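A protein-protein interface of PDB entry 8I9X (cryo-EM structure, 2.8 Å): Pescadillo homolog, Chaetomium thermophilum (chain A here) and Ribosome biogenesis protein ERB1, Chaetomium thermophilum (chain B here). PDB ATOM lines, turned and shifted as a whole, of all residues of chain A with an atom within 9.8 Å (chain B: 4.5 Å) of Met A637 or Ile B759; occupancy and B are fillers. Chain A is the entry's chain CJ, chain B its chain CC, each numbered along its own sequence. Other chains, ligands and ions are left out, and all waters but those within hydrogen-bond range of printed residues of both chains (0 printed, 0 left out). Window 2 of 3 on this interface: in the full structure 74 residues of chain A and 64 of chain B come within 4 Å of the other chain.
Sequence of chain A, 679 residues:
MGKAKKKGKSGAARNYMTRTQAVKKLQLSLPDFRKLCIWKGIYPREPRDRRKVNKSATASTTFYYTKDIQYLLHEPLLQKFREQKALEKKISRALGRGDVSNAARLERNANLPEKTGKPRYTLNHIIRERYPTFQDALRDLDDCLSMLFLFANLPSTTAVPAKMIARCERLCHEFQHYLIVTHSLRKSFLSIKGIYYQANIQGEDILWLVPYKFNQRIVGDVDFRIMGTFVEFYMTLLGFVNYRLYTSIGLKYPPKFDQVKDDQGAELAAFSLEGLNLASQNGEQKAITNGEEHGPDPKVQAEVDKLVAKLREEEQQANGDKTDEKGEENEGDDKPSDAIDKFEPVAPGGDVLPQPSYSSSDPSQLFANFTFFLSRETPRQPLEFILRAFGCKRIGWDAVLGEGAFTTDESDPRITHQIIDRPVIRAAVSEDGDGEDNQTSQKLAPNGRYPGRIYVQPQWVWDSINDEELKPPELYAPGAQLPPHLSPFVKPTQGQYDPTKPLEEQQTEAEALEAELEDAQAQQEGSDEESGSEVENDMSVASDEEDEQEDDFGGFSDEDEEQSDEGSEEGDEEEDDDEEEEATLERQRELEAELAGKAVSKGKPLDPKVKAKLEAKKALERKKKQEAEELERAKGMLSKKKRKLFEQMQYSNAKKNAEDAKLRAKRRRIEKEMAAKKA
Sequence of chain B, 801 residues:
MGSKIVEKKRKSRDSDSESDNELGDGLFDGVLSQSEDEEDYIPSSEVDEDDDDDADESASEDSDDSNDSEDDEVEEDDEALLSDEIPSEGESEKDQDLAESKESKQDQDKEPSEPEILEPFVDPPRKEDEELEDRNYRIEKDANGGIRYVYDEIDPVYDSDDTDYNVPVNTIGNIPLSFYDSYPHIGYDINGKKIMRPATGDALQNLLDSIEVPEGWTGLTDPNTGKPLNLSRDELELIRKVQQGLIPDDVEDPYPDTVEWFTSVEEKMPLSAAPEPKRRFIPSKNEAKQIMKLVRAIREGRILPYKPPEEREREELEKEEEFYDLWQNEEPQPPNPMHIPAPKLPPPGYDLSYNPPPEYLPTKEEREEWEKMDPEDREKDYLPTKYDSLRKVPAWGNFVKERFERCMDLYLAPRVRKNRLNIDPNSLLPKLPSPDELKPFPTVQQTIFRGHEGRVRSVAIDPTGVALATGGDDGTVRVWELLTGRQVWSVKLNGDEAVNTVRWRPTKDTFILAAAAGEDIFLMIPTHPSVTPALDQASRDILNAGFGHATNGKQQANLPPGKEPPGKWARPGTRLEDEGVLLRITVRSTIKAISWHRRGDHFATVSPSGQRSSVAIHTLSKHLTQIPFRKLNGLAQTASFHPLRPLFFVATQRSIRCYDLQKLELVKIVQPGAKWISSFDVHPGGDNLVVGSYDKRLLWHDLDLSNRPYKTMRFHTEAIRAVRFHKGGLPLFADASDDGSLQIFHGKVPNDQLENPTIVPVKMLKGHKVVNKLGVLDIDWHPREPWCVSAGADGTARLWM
CE1 of Phe B715 touches O of Glu A632 (3.5 Å).
Leu B432 touches Arg A633.
CE1 of Phe B715 touches O of Arg A633, at 3.2 Å.
Gly A636 touches Met B713.
Phe B715 touches Gly A636 (CZ to CA, 3.5 Å).
Pro B430 touches Met A637 (CG to CB, 3.7 Å).
Met A637 touches Thr B712 (O to O, 3.5 Å).
Met A637 touches Ile B759 (CE to O, 3.3 Å).
CE of Met A637 touches CD of Pro B761 (3.4 Å).
Leu A638 touches Thr B712 (O to O, 3.9 Å).
Of the 15 printed residues of chain A, 6 touch a printed residue of chain B.
Hydrophobic or aromatic side chains of chain A that line the printed part of chain B: Ala A634 and Met A637.
Printed residues of chain B that touch a printed residue of chain A: Pro B430, Leu B432, Thr B712, Met B713, Phe B715, Ile B759 and Pro B761.
Hydrophobic or aromatic side chains of chain B within 4 Å of the printed part of chain A: Pro B430, Leu B432, Met B713, Phe B715, Ile B759 and Pro B761.
Printed residues of chain B within 4 Å of Met A637: Pro B430 (3.7 Å), Thr B712 (3.5 Å), Met B713 (3.6 Å), Ile B759 (3.3 Å) and Pro B761 (3.4 Å).
No residue of chain A comes within 4 Å of Gly B747.
No residue of chain A comes within 4 Å of Thr B758.
Printed residues of chain A within 4 Å of Pro B761: Arg A633 (2.9 Å) and Met A637 (3.4 Å).
Printed residues of chain B within 4 Å of Leu A638: Thr B712.
Of the printed residues of chain B, Glu A632 touches Phe B715 (3.5 Å).
Printed residues of chain B within 4 Å of Gly A636: Met B713 (3.1 Å) and Phe B715 (3.5 Å).
Lys A635 touches none of the printed residues of chain B.
The nearest printed residue of chain B that does not touch Met A637 is Phe B715 (4.002 Å).
The side-chain sulfur (SD) of Met A637 lies close to the side-chain sulfur (SD) of Met B713, at 3.6 Å.
O of Pro B761 lies within hydrogen-bond range of NH1 of Arg A633 (2.9 Å).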
ATOM      1  N   GLU A 630       2.369 -19.309   3.054  1.00  0.00           N
ATOM      2  CA  GLU A 630       2.854 -20.553   2.461  1.00  0.00           C
ATOM      3  C   GLU A 630       3.740 -20.265   1.254  1.00  0.00           C
ATOM      4  O   GLU A 630       4.783 -20.909   1.048  1.00  0.00           O
ATOM      5  CB  GLU A 630       1.667 -21.430   2.059  1.00  0.00           C
ATOM      6  CG  GLU A 630       1.945 -22.925   2.059  1.00  0.00           C
ATOM      7  CD  GLU A 630       1.961 -23.527   3.451  1.00  0.00           C
ATOM      8  OE1 GLU A 630       1.837 -22.775   4.441  1.00  0.00           O
ATOM      9  OE2 GLU A 630       2.098 -24.765   3.555  1.00  0.00           O
ATOM     10  N   LEU A 631       3.332 -19.283   0.446  1.00  0.00           N
ATOM     11  CA  LEU A 631       4.087 -18.954  -0.755  1.00  0.00           C
ATOM     12  C   LEU A 631       5.480 -18.435  -0.419  1.00  0.00           C
ATOM     13  O   LEU A 631       6.462 -18.869  -1.028  1.00  0.00           O
ATOM     14  CB  LEU A 631       3.321 -17.938  -1.604  1.00  0.00           C
ATOM     15  CG  LEU A 631       3.945 -17.566  -2.949  1.00  0.00           C
ATOM     16  CD1 LEU A 631       4.063 -18.794  -3.835  1.00  0.00           C
ATOM     17  CD2 LEU A 631       3.127 -16.484  -3.634  1.00  0.00           C
ATOM     18  N   GLU A 632       5.598 -17.502   0.538  1.00  0.00           N
ATOM     19  CA  GLU A 632       6.954 -17.048   0.865  1.00  0.00           C
ATOM     20  C   GLU A 632       7.772 -18.169   1.490  1.00  0.00           C
ATOM     21  O   GLU A 632       8.980 -18.263   1.241  1.00  0.00           O
ATOM     22  CB  GLU A 632       7.042 -15.808   1.778  1.00  0.00           C
ATOM     23  CG  GLU A 632       6.564 -14.454   1.231  1.00  0.00           C
ATOM     24  CD  GLU A 632       5.094 -14.227   1.362  1.00  0.00           C
ATOM     25  OE1 GLU A 632       4.446 -15.092   1.953  1.00  0.00           O
ATOM     26  OE2 GLU A 632       4.593 -13.187   0.885  1.00  0.00           O
ATOM     27  N   ARG A 633       7.138 -19.048   2.234  1.00  0.00           N
ATOM     28  CA  ARG A 633       7.955 -20.076   2.913  1.00  0.00           C
ATOM     29  C   ARG A 633       8.628 -20.945   1.859  1.00  0.00           C
ATOM     30  O   ARG A 633       9.858 -21.125   1.932  1.00  0.00           O
ATOM     31  CB  ARG A 633       7.080 -20.927   3.832  1.00  0.00           C
ATOM     32  CG  ARG A 633       7.044 -20.463   5.280  1.00  0.00           C
ATOM     33  CD  ARG A 633       5.816 -20.991   5.997  1.00  0.00           C
ATOM     34  NE  ARG A 633       5.591 -22.415   5.790  1.00  0.00           N
ATOM     35  CZ  ARG A 633       5.976 -23.375   6.622  1.00  0.00           C
ATOM     36  NH1 ARG A 633       6.613 -23.072   7.740  1.00  0.00           N
ATOM     37  NH2 ARG A 633       5.717 -24.638   6.337  1.00  0.00           N
ATOM     38  N   ALA A 634       7.860 -21.455   0.908  1.00  0.00           N
ATOM     39  CA  ALA A 634       8.434 -22.388  -0.080  1.00  0.00           C
ATOM     40  C   ALA A 634       9.442 -21.672  -0.973  1.00  0.00           C
ATOM     41  O   ALA A 634      10.486 -22.268  -1.259  1.00  0.00           O
ATOM     42  CB  ALA A 634       7.321 -22.993  -0.887  1.00  0.00           C
ATOM     43  N   LYS A 635       9.152 -20.441  -1.379  1.00  0.00           N
ATOM     44  CA  LYS A 635      10.015 -19.681  -2.312  1.00  0.00           C
ATOM     45  C   LYS A 635      11.407 -19.511  -1.719  1.00  0.00           C
ATOM     46  O   LYS A 635      12.358 -19.374  -2.500  1.00  0.00           O
ATOM     47  CB  LYS A 635       9.358 -18.325  -2.532  1.00  0.00           C
ATOM     48  CG  LYS A 635       9.711 -17.575  -3.805  1.00  0.00           C
ATOM     49  CD  LYS A 635       8.693 -16.494  -4.085  1.00  0.00           C
ATOM     50  CE  LYS A 635       9.115 -15.523  -5.166  1.00  0.00           C
ATOM     51  NZ  LYS A 635      10.203 -14.631  -4.702  1.00  0.00           N
ATOM     52  N   GLY A 636      11.523 -19.513  -0.401  1.00  0.00           N
ATOM     53  CA  GLY A 636      12.829 -19.244   0.213  1.00  0.00           C
ATOM     54  C   GLY A 636      13.747 -20.438   0.199  1.00  0.00           C
ATOM     55  O   GLY A 636      14.957 -20.241   0.306  1.00  0.00           O
ATOM     56  N   MET A 637      13.189 -21.632   0.085  1.00  0.00           N
ATOM     57  CA  MET A 637      14.036 -22.828  -0.017  1.00  0.00           C
ATOM     58  C   MET A 637      14.494 -23.031  -1.462  1.00  0.00           C
ATOM     59  O   MET A 637      15.387 -23.853  -1.672  1.00  0.00           O
ATOM     60  CB  MET A 637      13.240 -24.038   0.456  1.00  0.00           C
ATOM     61  CG  MET A 637      13.084 -24.094   1.953  1.00  0.00           C
ATOM     62  SD  MET A 637      14.456 -24.999   2.687  1.00  0.00           S
ATOM     63  CE  MET A 637      14.308 -24.472   4.390  1.00  0.00           C
ATOM     64  N   LEU A 638      13.916 -22.312  -2.419  1.00  0.00           N
ATOM     65  CA  LEU A 638      14.277 -22.474  -3.857  1.00  0.00           C
ATOM     66  C   LEU A 638      15.664 -21.886  -4.120  1.00  0.00           C
ATOM     67  O   LEU A 638      16.131 -21.079  -3.299  1.00  0.00           O
ATOM     68  CB  LEU A 638      13.239 -21.798  -4.750  1.00  0.00           C
ATOM     69  CG  LEU A 638      12.125 -22.695  -5.276  1.00  0.00           C
ATOM     70  CD1 LEU A 638      11.363 -21.980  -6.377  1.00  0.00           C
ATOM     71  CD2 LEU A 638      12.686 -24.007  -5.794  1.00  0.00           C
ATOM     72  N   SER A 639      16.283 -22.254  -5.235  1.00  0.00           N
ATOM     73  CA  SER A 639      17.663 -21.799  -5.558  1.00  0.00           C
ATOM     74  C   SER A 639      17.637 -20.464  -6.281  1.00  0.00           C
ATOM     75  O   SER A 639      16.559 -20.046  -6.667  1.00  0.00           O
ATOM     76  CB  SER A 639      18.375 -22.817  -6.372  1.00  0.00           C
ATOM     77  OG  SER A 639      17.954 -22.772  -7.725  1.00  0.00           O
ATOM     78  N   LYS A 640      18.792 -19.848  -6.499  1.00  0.00           N
ATOM     79  CA  LYS A 640      18.815 -18.489  -7.077  1.00  0.00           C
ATOM     80  C   LYS A 640      18.225 -18.527  -8.487  1.00  0.00           C
ATOM     81  O   LYS A 640      17.376 -17.672  -8.770  1.00  0.00           O
ATOM     82  CB  LYS A 640      20.255 -17.983  -7.000  1.00  0.00           C
ATOM     83  CG  LYS A 640      20.445 -16.475  -7.036  1.00  0.00           C
ATOM     84  CD  LYS A 640      21.834 -16.068  -6.604  1.00  0.00           C
ATOM     85  CE  LYS A 640      22.102 -14.587  -6.766  1.00  0.00           C
ATOM     86  NZ  LYS A 640      23.490 -14.236  -6.385  1.00  0.00           N
ATOM     87  N   LYS A 641      18.612 -19.513  -9.304  1.00  0.00           N
ATOM     88  CA  LYS A 641      18.163 -19.598 -10.711  1.00  0.00           C
ATOM     89  C   LYS A 641      16.731 -20.125 -10.767  1.00  0.00           C
ATOM     90  O   LYS A 641      15.957 -19.607 -11.586  1.00  0.00           O
ATOM     91  CB  LYS A 641      19.168 -20.442 -11.494  1.00  0.00           C
ATOM     92  CG  LYS A 641      20.568 -19.842 -11.564  1.00  0.00           C
ATOM     93  CD  LYS A 641      21.519 -20.552 -12.500  1.00  0.00           C
ATOM     94  CE  LYS A 641      21.321 -20.170 -13.949  1.00  0.00           C
ATOM     95  NZ  LYS A 641      22.418 -20.683 -14.801  1.00  0.00           N
ATOM     96  N   LYS A 642      16.389 -21.095  -9.925  1.00  0.00           N
ATOM     97  CA  LYS A 642      15.016 -21.650  -9.890  1.00  0.00           C
ATOM     98  C   LYS A 642      14.088 -20.623  -9.253  1.00  0.00           C
ATOM     99  O   LYS A 642      12.912 -20.603  -9.645  1.00  0.00           O
ATOM    100  CB  LYS A 642      14.969 -22.972  -9.124  1.00  0.00           C
ATOM    101  CG  LYS A 642      14.466 -24.167  -9.918  1.00  0.00           C
ATOM    102  CD  LYS A 642      14.517 -25.455  -9.132  1.00  0.00           C
ATOM    103  CE  LYS A 642      13.980 -26.645  -9.897  1.00  0.00           C
ATOM    104  NZ  LYS A 642      14.731 -26.876 -11.155  1.00  0.00           N
ATOM    105  N   ARG A 643      14.587 -19.790  -8.353  1.00  0.00           N
ATOM    106  CA  ARG A 643      13.728 -18.714  -7.819  1.00  0.00           C
ATOM    107  C   ARG A 643      13.436 -17.741  -8.955  1.00  0.00           C
ATOM    108  O   ARG A 643      12.267 -17.363  -9.104  1.00  0.00           O
ATOM    109  CB  ARG A 643      14.418 -17.924  -6.713  1.00  0.00           C
ATOM    110  CG  ARG A 643      13.471 -17.184  -5.783  1.00  0.00           C
ATOM    111  CD  ARG A 643      14.278 -16.341  -4.820  1.00  0.00           C
ATOM    112  NE  ARG A 643      13.466 -15.374  -4.101  1.00  0.00           N
ATOM    113  CZ  ARG A 643      13.046 -15.525  -2.855  1.00  0.00           C
ATOM    114  NH1 ARG A 643      13.367 -16.612  -2.174  1.00  0.00           N
ATOM    115  NH2 ARG A 643      12.313 -14.586  -2.287  1.00  0.00           N
ATOM    116  N   PHE A 646      10.789 -18.937 -11.293  1.00  0.00           N
ATOM    117  CA  PHE A 646       9.429 -18.935 -10.708  1.00  0.00           C
ATOM    118  C   PHE A 646       8.894 -17.513 -10.659  1.00  0.00           C
ATOM    119  O   PHE A 646       7.693 -17.324 -10.871  1.00  0.00           O
ATOM    120  CB  PHE A 646       9.467 -19.539  -9.312  1.00  0.00           C
ATOM    121  CG  PHE A 646       8.182 -19.475  -8.531  1.00  0.00           C
ATOM    122  CD1 PHE A 646       8.017 -18.549  -7.516  1.00  0.00           C
ATOM    123  CD2 PHE A 646       7.147 -20.352  -8.799  1.00  0.00           C
ATOM    124  CE1 PHE A 646       6.840 -18.493  -6.791  1.00  0.00           C
ATOM    125  CE2 PHE A 646       5.968 -20.292  -8.074  1.00  0.00           C
ATOM    126  CZ  PHE A 646       5.817 -19.365  -7.073  1.00  0.00           C
ATOM    127  N   PRO B 430       9.055 -26.313  -3.179  1.00  0.00           N
ATOM    128  CA  PRO B 430       9.202 -27.463  -2.282  1.00  0.00           C
ATOM    129  C   PRO B 430       7.966 -27.718  -1.402  1.00  0.00           C
ATOM    130  O   PRO B 430       7.233 -26.785  -1.161  1.00  0.00           O
ATOM    131  CB  PRO B 430      10.377 -27.054  -1.391  1.00  0.00           C
ATOM    132  CG  PRO B 430      10.395 -25.555  -1.442  1.00  0.00           C
ATOM    133  CD  PRO B 430       9.969 -25.222  -2.853  1.00  0.00           C
ATOM    134  N   LEU B 432       6.410 -28.414   2.283  1.00  0.00           N
ATOM    135  CA  LEU B 432       6.944 -28.134   3.604  1.00  0.00           C
ATOM    136  C   LEU B 432       5.969 -28.572   4.690  1.00  0.00           C
ATOM    137  O   LEU B 432       4.771 -28.280   4.602  1.00  0.00           O
ATOM    138  CB  LEU B 432       7.252 -26.638   3.777  1.00  0.00           C
ATOM    139  CG  LEU B 432       8.596 -26.087   3.286  1.00  0.00           C
ATOM    140  CD1 LEU B 432       9.753 -26.724   4.045  1.00  0.00           C
ATOM    141  CD2 LEU B 432       8.776 -26.250   1.781  1.00  0.00           C
ATOM    142  N   TRP B 700      23.256 -24.025   4.368  1.00  0.00           N
ATOM    143  CA  TRP B 700      23.565 -25.144   5.246  1.00  0.00           C
ATOM    144  C   TRP B 700      24.492 -26.118   4.539  1.00  0.00           C
ATOM    145  O   TRP B 700      24.193 -26.608   3.443  1.00  0.00           O
ATOM    146  CB  TRP B 700      22.295 -25.836   5.752  1.00  0.00           C
ATOM    147  CG  TRP B 700      22.546 -26.909   6.803  1.00  0.00           C
ATOM    148  CD1 TRP B 700      23.490 -27.895   6.764  1.00  0.00           C
ATOM    149  CD2 TRP B 700      21.932 -27.007   8.096  1.00  0.00           C
ATOM    150  NE1 TRP B 700      23.446 -28.646   7.908  1.00  0.00           N
ATOM    151  CE2 TRP B 700      22.506 -28.114   8.749  1.00  0.00           C
ATOM    152  CE3 TRP B 700      20.939 -26.282   8.754  1.00  0.00           C
ATOM    153  CZ2 TRP B 700      22.116 -28.515  10.024  1.00  0.00           C
ATOM    154  CZ3 TRP B 700      20.558 -26.681  10.023  1.00  0.00           C
ATOM    155  CH2 TRP B 700      21.139 -27.789  10.641  1.00  0.00           C
ATOM    156  N   LYS B 711      22.314 -26.963   1.147  1.00  0.00           N
ATOM    157  CA  LYS B 711      20.990 -26.313   0.918  1.00  0.00           C
ATOM    158  C   LYS B 711      21.118 -24.792   1.056  1.00  0.00           C
ATOM    159  O   LYS B 711      21.745 -24.353   2.029  1.00  0.00           O
ATOM    160  CB  LYS B 711      19.973 -26.799   1.944  1.00  0.00           C
ATOM    161  CG  LYS B 711      18.524 -26.449   1.638  1.00  0.00           C
ATOM    162  CD  LYS B 711      17.844 -27.454   0.740  1.00  0.00           C
ATOM    163  CE  LYS B 711      17.625 -28.791   1.417  1.00  0.00           C
ATOM    164  NZ  LYS B 711      16.757 -28.664   2.611  1.00  0.00           N
ATOM    165  N   THR B 712      20.542 -24.023   0.127  1.00  0.00           N
ATOM    166  CA  THR B 712      20.615 -22.539   0.195  1.00  0.00           C
ATOM    167  C   THR B 712      19.224 -21.941   0.396  1.00  0.00           C
ATOM    168  O   THR B 712      18.296 -22.381  -0.302  1.00  0.00           O
ATOM    169  CB  THR B 712      21.296 -21.945  -1.040  1.00  0.00           C
ATOM    170  OG1 THR B 712      20.537 -22.309  -2.194  1.00  0.00           O
ATOM    171  CG2 THR B 712      22.727 -22.407  -1.206  1.00  0.00           C
ATOM    172  N   MET B 713      19.086 -20.983   1.315  1.00  0.00           N
ATOM    173  CA  MET B 713      17.768 -20.397   1.626  1.00  0.00           C
ATOM    174  C   MET B 713      17.802 -18.876   1.539  1.00  0.00           C
ATOM    175  O   MET B 713      18.782 -18.295   2.027  1.00  0.00           O
ATOM    176  CB  MET B 713      17.379 -20.754   3.055  1.00  0.00           C
ATOM    177  CG  MET B 713      16.554 -21.999   3.179  1.00  0.00           C
ATOM    178  SD  MET B 713      17.596 -23.439   3.441  1.00  0.00           S
ATOM    179  CE  MET B 713      18.542 -22.915   4.868  1.00  0.00           C
ATOM    180  N   PHE B 715      15.250 -15.654   2.545  1.00  0.00           N
ATOM    181  CA  PHE B 715      14.002 -15.188   3.132  1.00  0.00           C
ATOM    182  C   PHE B 715      14.037 -13.705   3.469  1.00  0.00           C
ATOM    183  O   PHE B 715      13.062 -13.188   4.026  1.00  0.00           O
ATOM    184  CB  PHE B 715      13.674 -15.989   4.393  1.00  0.00           C
ATOM    185  CG  PHE B 715      13.195 -17.377   4.118  1.00  0.00           C
ATOM    186  CD1 PHE B 715      11.857 -17.631   3.877  1.00  0.00           C
ATOM    187  CD2 PHE B 715      14.087 -18.430   4.095  1.00  0.00           C
ATOM    188  CE1 PHE B 715      11.420 -18.913   3.628  1.00  0.00           C
ATOM    189  CE2 PHE B 715      13.656 -19.705   3.844  1.00  0.00           C
ATOM    190  CZ  PHE B 715      12.321 -19.951   3.612  1.00  0.00           C
ATOM    191  N   PHE B 733      17.286 -23.061  14.784  1.00  0.00           N
ATOM    192  CA  PHE B 733      18.383 -22.112  14.421  1.00  0.00           C
ATOM    193  C   PHE B 733      17.806 -20.776  13.954  1.00  0.00           C
ATOM    194  O   PHE B 733      16.769 -20.771  13.290  1.00  0.00           O
ATOM    195  CB  PHE B 733      19.405 -22.695  13.443  1.00  0.00           C
ATOM    196  CG  PHE B 733      18.966 -23.120  12.067  1.00  0.00           C
ATOM    197  CD1 PHE B 733      18.270 -24.300  11.871  1.00  0.00           C
ATOM    198  CD2 PHE B 733      19.351 -22.392  10.954  1.00  0.00           C
ATOM    199  CE1 PHE B 733      17.908 -24.703  10.595  1.00  0.00           C
ATOM    200  CE2 PHE B 733      18.993 -22.797   9.680  1.00  0.00           C
ATOM    201  CZ  PHE B 733      18.275 -23.954   9.502  1.00  0.00           C
ATOM    202  N   HIS B 746      13.710 -24.587  11.756  1.00  0.00           N
ATOM    203  CA  HIS B 746      13.854 -25.886  12.396  1.00  0.00           C
ATOM    204  C   HIS B 746      14.867 -26.725  11.632  1.00  0.00           C
ATOM    205  O   HIS B 746      14.714 -26.961  10.431  1.00  0.00           O
ATOM    206  CB  HIS B 746      12.524 -26.634  12.449  1.00  0.00           C
ATOM    207  CG  HIS B 746      12.671 -28.103  12.695  1.00  0.00           C
ATOM    208  ND1 HIS B 746      12.339 -29.051  11.753  1.00  0.00           N
ATOM    209  CD2 HIS B 746      13.104 -28.786  13.779  1.00  0.00           C
ATOM    210  CE1 HIS B 746      12.567 -30.256  12.244  1.00  0.00           C
ATOM    211  NE2 HIS B 746      13.031 -30.123  13.472  1.00  0.00           N
ATOM    212  N   GLY B 747      15.900 -27.174  12.336  1.00  0.00           N
ATOM    213  CA  GLY B 747      16.878 -28.064  11.746  1.00  0.00           C
ATOM    214  C   GLY B 747      17.086 -29.316  12.569  1.00  0.00           C
ATOM    215  O   GLY B 747      17.597 -29.249  13.690  1.00  0.00           O
ATOM    216  N   PRO B 757      19.644 -34.205   6.928  1.00  0.00           N
ATOM    217  CA  PRO B 757      18.833 -33.377   7.825  1.00  0.00           C
ATOM    218  C   PRO B 757      17.720 -32.659   7.077  1.00  0.00           C
ATOM    219  O   PRO B 757      17.857 -32.280   5.912  1.00  0.00           O
ATOM    220  CB  PRO B 757      19.848 -32.381   8.398  1.00  0.00           C
ATOM    221  CG  PRO B 757      21.150 -33.098   8.300  1.00  0.00           C
ATOM    222  CD  PRO B 757      21.070 -33.850   7.005  1.00  0.00           C
ATOM    223  N   THR B 758      16.601 -32.474   7.770  1.00  0.00           N
ATOM    224  CA  THR B 758      15.425 -31.809   7.223  1.00  0.00           C
ATOM    225  C   THR B 758      15.382 -30.384   7.754  1.00  0.00           C
ATOM    226  O   THR B 758      15.501 -30.167   8.964  1.00  0.00           O
ATOM    227  CB  THR B 758      14.146 -32.557   7.592  1.00  0.00           C
ATOM    228  OG1 THR B 758      13.788 -32.250   8.945  1.00  0.00           O
ATOM    229  CG2 THR B 758      14.348 -34.057   7.453  1.00  0.00           C
ATOM    230  N   ILE B 759      15.212 -29.421   6.854  1.00  0.00           N
ATOM    231  CA  ILE B 759      15.298 -28.006   7.193  1.00  0.00           C
ATOM    232  C   ILE B 759      13.964 -27.361   6.857  1.00  0.00           C
ATOM    233  O   ILE B 759      13.527 -27.388   5.699  1.00  0.00           O
ATOM    234  CB  ILE B 759      16.446 -27.311   6.456  1.00  0.00           C
ATOM    235  CG1 ILE B 759      17.753 -28.007   6.813  1.00  0.00           C
ATOM    236  CG2 ILE B 759      16.497 -25.842   6.827  1.00  0.00           C
ATOM    237  CD1 ILE B 759      18.053 -27.951   8.270  1.00  0.00           C
ATOM    238  N   VAL B 760      13.314 -26.784   7.862  1.00  0.00           N
ATOM    239  CA  VAL B 760      12.001 -26.169   7.690  1.00  0.00           C
ATOM    240  C   VAL B 760      11.947 -24.856   8.460  1.00  0.00           C
ATOM    241  O   VAL B 760      12.113 -24.854   9.688  1.00  0.00           O
ATOM    242  CB  VAL B 760      10.878 -27.109   8.157  1.00  0.00           C
ATOM    243  CG1 VAL B 760       9.534 -26.403   8.078  1.00  0.00           C
ATOM    244  CG2 VAL B 760      10.867 -28.379   7.330  1.00  0.00           C
ATOM    245  N   PRO B 761      11.730 -23.725   7.794  1.00  0.00           N
ATOM    246  CA  PRO B 761      11.467 -22.484   8.529  1.00  0.00           C
ATOM    247  C   PRO B 761      10.199 -22.611   9.353  1.00  0.00           C
ATOM    248  O   PRO B 761       9.226 -23.239   8.931  1.00  0.00           O
ATOM    249  CB  PRO B 761      11.322 -21.440   7.417  1.00  0.00           C
ATOM    250  CG  PRO B 761      10.963 -22.236   6.205  1.00  0.00           C
ATOM    251  CD  PRO B 761      11.731 -23.509   6.340  1.00  0.00           C
